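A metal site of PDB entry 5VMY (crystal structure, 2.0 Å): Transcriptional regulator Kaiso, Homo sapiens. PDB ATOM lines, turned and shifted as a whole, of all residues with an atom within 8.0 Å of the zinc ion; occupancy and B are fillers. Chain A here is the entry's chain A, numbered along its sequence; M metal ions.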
ATOM      1  N   PRO A  53     -17.555  28.170   0.535  1.00  0.00           N
ATOM      2  CA  PRO A  53     -18.521  27.231   1.112  1.00  0.00           C
ATOM      3  C   PRO A  53     -18.319  25.798   0.629  1.00  0.00           C
ATOM      4  O   PRO A  53     -18.028  25.606  -0.552  1.00  0.00           O
ATOM      5  CB  PRO A  53     -19.861  27.776   0.622  1.00  0.00           C
ATOM      6  CG  PRO A  53     -19.525  28.437  -0.673  1.00  0.00           C
ATOM      7  CD  PRO A  53     -18.152  29.022  -0.502  1.00  0.00           C
ATOM      8  N   CYS A  54     -18.451  24.817   1.532  1.00  0.00           N
ATOM      9  CA  CYS A  54     -18.375  23.400   1.160  1.00  0.00           C
ATOM     10  C   CYS A  54     -19.513  23.112   0.199  1.00  0.00           C
ATOM     11  O   CYS A  54     -20.641  23.564   0.387  1.00  0.00           O
ATOM     12  CB  CYS A  54     -18.460  22.482   2.381  1.00  0.00           C
ATOM     13  SG  CYS A  54     -18.644  20.656   2.017  1.00  0.00           S
ATOM     14  N   ARG A  55     -19.232  22.364  -0.856  1.00  0.00           N
ATOM     15  CA  ARG A  55     -20.298  22.116  -1.812  1.00  0.00           C
ATOM     16  C   ARG A  55     -21.057  20.816  -1.528  1.00  0.00           C
ATOM     17  O   ARG A  55     -21.871  20.405  -2.347  1.00  0.00           O
ATOM     18  CB  ARG A  55     -19.741  22.151  -3.232  1.00  0.00           C
ATOM     19  CG  ARG A  55     -19.721  23.608  -3.746  1.00  0.00           C
ATOM     20  CD  ARG A  55     -18.498  23.963  -4.567  1.00  0.00           C
ATOM     21  NE  ARG A  55     -17.248  23.560  -3.952  1.00  0.00           N
ATOM     22  CZ  ARG A  55     -16.049  23.793  -4.473  1.00  0.00           C
ATOM     23  NH1 ARG A  55     -15.958  24.466  -5.624  1.00  0.00           N
ATOM     24  NH2 ARG A  55     -14.957  23.377  -3.876  1.00  0.00           N
ATOM     25  N   TYR A  56     -20.832  20.239  -0.357  1.00  0.00           N
ATOM     26  CA  TYR A  56     -21.556  19.038   0.065  1.00  0.00           C
ATOM     27  C   TYR A  56     -22.311  19.246   1.377  1.00  0.00           C
ATOM     28  O   TYR A  56     -23.200  18.465   1.716  1.00  0.00           O
ATOM     29  CB  TYR A  56     -20.605  17.845   0.235  1.00  0.00           C
ATOM     30  CG  TYR A  56     -19.820  17.511  -0.990  1.00  0.00           C
ATOM     31  CD1 TYR A  56     -20.309  16.604  -1.928  1.00  0.00           C
ATOM     32  CD2 TYR A  56     -18.585  18.083  -1.224  1.00  0.00           C
ATOM     33  CE1 TYR A  56     -19.580  16.291  -3.058  1.00  0.00           C
ATOM     34  CE2 TYR A  56     -17.855  17.779  -2.350  1.00  0.00           C
ATOM     35  CZ  TYR A  56     -18.360  16.887  -3.258  1.00  0.00           C
ATOM     36  OH  TYR A  56     -17.620  16.580  -4.382  1.00  0.00           O
ATOM     37  N   CYS A  57     -21.951  20.273   2.125  1.00  0.00           N
ATOM     38  CA  CYS A  57     -22.678  20.586   3.354  1.00  0.00           C
ATOM     39  C   CYS A  57     -22.700  22.084   3.613  1.00  0.00           C
ATOM     40  O   CYS A  57     -22.302  22.878   2.747  1.00  0.00           O
ATOM     41  CB  CYS A  57     -22.057  19.860   4.554  1.00  0.00           C
ATOM     42  SG  CYS A  57     -20.568  20.630   5.197  1.00  0.00           S
ATOM     43  N   GLU A  58     -23.144  22.463   4.809  1.00  0.00           N
ATOM     44  CA  GLU A  58     -23.352  23.867   5.184  1.00  0.00           C
ATOM     45  C   GLU A  58     -22.067  24.665   5.388  1.00  0.00           C
ATOM     46  O   GLU A  58     -22.078  25.883   5.250  1.00  0.00           O
ATOM     47  CB  GLU A  58     -24.183  23.946   6.468  1.00  0.00           C
ATOM     48  CG  GLU A  58     -25.580  23.396   6.331  1.00  0.00           C
ATOM     49  CD  GLU A  58     -26.371  24.100   5.250  1.00  0.00           C
ATOM     50  OE1 GLU A  58     -26.240  25.329   5.112  1.00  0.00           O
ATOM     51  OE2 GLU A  58     -27.131  23.417   4.533  1.00  0.00           O
ATOM     52  N   LYS A  59     -20.976  23.976   5.739  1.00  0.00           N
ATOM     53  CA  LYS A  59     -19.763  24.645   6.223  1.00  0.00           C
ATOM     54  C   LYS A  59     -19.189  25.672   5.241  1.00  0.00           C
ATOM     55  O   LYS A  59     -19.268  25.510   4.031  1.00  0.00           O
ATOM     56  CB  LYS A  59     -18.680  23.627   6.552  1.00  0.00           C
ATOM     57  CG  LYS A  59     -18.823  22.959   7.915  1.00  0.00           C
ATOM     58  CD  LYS A  59     -17.594  22.100   8.207  1.00  0.00           C
ATOM     59  CE  LYS A  59     -17.558  21.614   9.650  1.00  0.00           C
ATOM     60  NZ  LYS A  59     -18.667  20.674   9.955  1.00  0.00           N
ATOM     61  N   VAL A  60     -18.590  26.727   5.787  1.00  0.00           N
ATOM     62  CA  VAL A  60     -17.967  27.759   4.967  1.00  0.00           C
ATOM     63  C   VAL A  60     -16.593  28.127   5.531  1.00  0.00           C
ATOM     64  O   VAL A  60     -16.444  28.337   6.724  1.00  0.00           O
ATOM     65  CB  VAL A  60     -18.857  29.010   4.890  1.00  0.00           C
ATOM     66  CG1 VAL A  60     -18.184  30.086   4.044  1.00  0.00           C
ATOM     67  CG2 VAL A  60     -20.228  28.662   4.332  1.00  0.00           C
ATOM     68  N   PHE A  61     -15.593  28.193   4.653  1.00  0.00           N
ATOM     69  CA  PHE A  61     -14.203  28.393   5.069  1.00  0.00           C
ATOM     70  C   PHE A  61     -13.604  29.714   4.588  1.00  0.00           C
ATOM     71  O   PHE A  61     -14.038  30.241   3.570  1.00  0.00           O
ATOM     72  CB  PHE A  61     -13.345  27.211   4.561  1.00  0.00           C
ATOM     73  CG  PHE A  61     -13.841  25.875   5.009  1.00  0.00           C
ATOM     74  CD1 PHE A  61     -14.847  25.212   4.307  1.00  0.00           C
ATOM     75  CD2 PHE A  61     -13.330  25.288   6.150  1.00  0.00           C
ATOM     76  CE1 PHE A  61     -15.322  23.984   4.736  1.00  0.00           C
ATOM     77  CE2 PHE A  61     -13.796  24.058   6.582  1.00  0.00           C
ATOM     78  CZ  PHE A  61     -14.797  23.407   5.873  1.00  0.00           C
ATOM     79  N   ARG A  67     -11.266  24.558   2.551  1.00  0.00           N
ATOM     80  CA  ARG A  67     -12.423  23.945   1.927  1.00  0.00           C
ATOM     81  C   ARG A  67     -12.050  22.658   1.171  1.00  0.00           C
ATOM     82  O   ARG A  67     -12.722  21.624   1.305  1.00  0.00           O
ATOM     83  CB  ARG A  67     -13.092  24.910   0.969  1.00  0.00           C
ATOM     84  CG  ARG A  67     -14.195  24.183   0.181  1.00  0.00           C
ATOM     85  CD  ARG A  67     -14.968  25.102  -0.684  1.00  0.00           C
ATOM     86  NE  ARG A  67     -14.182  25.683  -1.759  1.00  0.00           N
ATOM     87  CZ  ARG A  67     -14.688  26.544  -2.630  1.00  0.00           C
ATOM     88  NH1 ARG A  67     -15.961  26.891  -2.544  1.00  0.00           N
ATOM     89  NH2 ARG A  67     -13.924  27.050  -3.589  1.00  0.00           N
ATOM     90  N   HIS A  70     -11.373  19.751   3.339  1.00  0.00           N
ATOM     91  CA  HIS A  70     -12.643  19.340   3.920  1.00  0.00           C
ATOM     92  C   HIS A  70     -13.483  18.528   2.943  1.00  0.00           C
ATOM     93  O   HIS A  70     -14.124  17.547   3.332  1.00  0.00           O
ATOM     94  CB  HIS A  70     -13.423  20.567   4.380  1.00  0.00           C
ATOM     95  CG  HIS A  70     -14.841  20.255   4.746  1.00  0.00           C
ATOM     96  ND1 HIS A  70     -15.178  19.619   5.926  1.00  0.00           N
ATOM     97  CD2 HIS A  70     -16.004  20.460   4.079  1.00  0.00           C
ATOM     98  CE1 HIS A  70     -16.492  19.484   5.982  1.00  0.00           C
ATOM     99  NE2 HIS A  70     -17.022  19.997   4.881  1.00  0.00           N
ATOM    100  N   GLU A  71     -13.503  18.946   1.675  1.00  0.00           N
ATOM    101  CA  GLU A  71     -14.350  18.275   0.688  1.00  0.00           C
ATOM    102  C   GLU A  71     -13.838  16.881   0.382  1.00  0.00           C
ATOM    103  O   GLU A  71     -14.615  15.994   0.056  1.00  0.00           O
ATOM    104  CB  GLU A  71     -14.459  19.112  -0.592  1.00  0.00           C
ATOM    105  CG  GLU A  71     -15.422  20.302  -0.405  1.00  0.00           C
ATOM    106  CD  GLU A  71     -15.550  21.160  -1.643  1.00  0.00           C
ATOM    107  OE1 GLU A  71     -14.654  21.121  -2.509  1.00  0.00           O
ATOM    108  OE2 GLU A  71     -16.574  21.884  -1.763  1.00  0.00           O
ATOM    109  N   ILE A  72     -12.528  16.687   0.503  1.00  0.00           N
ATOM    110  CA  ILE A  72     -11.979  15.343   0.323  1.00  0.00           C
ATOM    111  C   ILE A  72     -12.523  14.378   1.398  1.00  0.00           C
ATOM    112  O   ILE A  72     -12.755  13.195   1.128  1.00  0.00           O
ATOM    113  CB  ILE A  72     -10.440  15.391   0.305  1.00  0.00           C
ATOM    114  CG1 ILE A  72     -10.000  15.757  -1.105  1.00  0.00           C
ATOM    115  CG2 ILE A  72      -9.829  14.041   0.661  1.00  0.00           C
ATOM    116  CD1 ILE A  72      -8.528  15.839  -1.302  1.00  0.00           C
ATOM    117  N   HIS A  73     -12.780  14.884   2.607  1.00  0.00           N
ATOM    118  CA  HIS A  73     -13.445  14.052   3.617  1.00  0.00           C
ATOM    119  C   HIS A  73     -14.822  13.554   3.172  1.00  0.00           C
ATOM    120  O   HIS A  73     -15.240  12.451   3.512  1.00  0.00           O
ATOM    121  CB  HIS A  73     -13.570  14.801   4.937  1.00  0.00           C
ATOM    122  CG  HIS A  73     -12.376  14.649   5.827  1.00  0.00           C
ATOM    123  ND1 HIS A  73     -11.266  15.468   5.742  1.00  0.00           N
ATOM    124  CD2 HIS A  73     -12.103  13.764   6.814  1.00  0.00           C
ATOM    125  CE1 HIS A  73     -10.372  15.102   6.642  1.00  0.00           C
ATOM    126  NE2 HIS A  73     -10.861  14.068   7.302  1.00  0.00           N
ATOM    127  N   HIS A  74     -15.545  14.377   2.421  1.00  0.00           N
ATOM    128  CA  HIS A  74     -16.842  13.959   1.883  1.00  0.00           C
ATOM    129  C   HIS A  74     -16.733  12.811   0.870  1.00  0.00           C
ATOM    130  O   HIS A  74     -17.543  11.890   0.873  1.00  0.00           O
ATOM    131  CB  HIS A  74     -17.553  15.158   1.244  1.00  0.00           C
ATOM    132  CG  HIS A  74     -18.211  16.078   2.228  1.00  0.00           C
ATOM    133  ND1 HIS A  74     -19.280  15.683   3.006  1.00  0.00           N
ATOM    134  CD2 HIS A  74     -17.994  17.379   2.534  1.00  0.00           C
ATOM    135  CE1 HIS A  74     -19.690  16.706   3.746  1.00  0.00           C
ATOM    136  NE2 HIS A  74     -18.930  17.750   3.472  1.00  0.00           N
HETATM  137 ZN    ZN M   1     -18.831  19.773   3.955  1.00  0.00          ZN
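The zinc ion is bound by a ring nitrogen (NE2) of His 70, a ring nitrogen (NE2) of His 74, the side-chain sulfur of Cys 54 and the side-chain sulfur of Cys 57.
The zinc ion has four donor atoms within binding distance.
The side-chain sulfur (SG) of Cys 54 lies close to the backbone NH (N) of Tyr 56 (3.3 Å).
N of Cys 54 is in hydrogen-bond range of O of Lys 59.
N of Lys 59 lies close to SG of Cys 57, at 3.4 Å.
Four residues have an atom within 4 Å of the zinc ion: Cys 54, Cys 57, His 70 and His 74.
The nearest printed residue that does not touch the zinc ion is Tyr 56 (4.4 Å).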
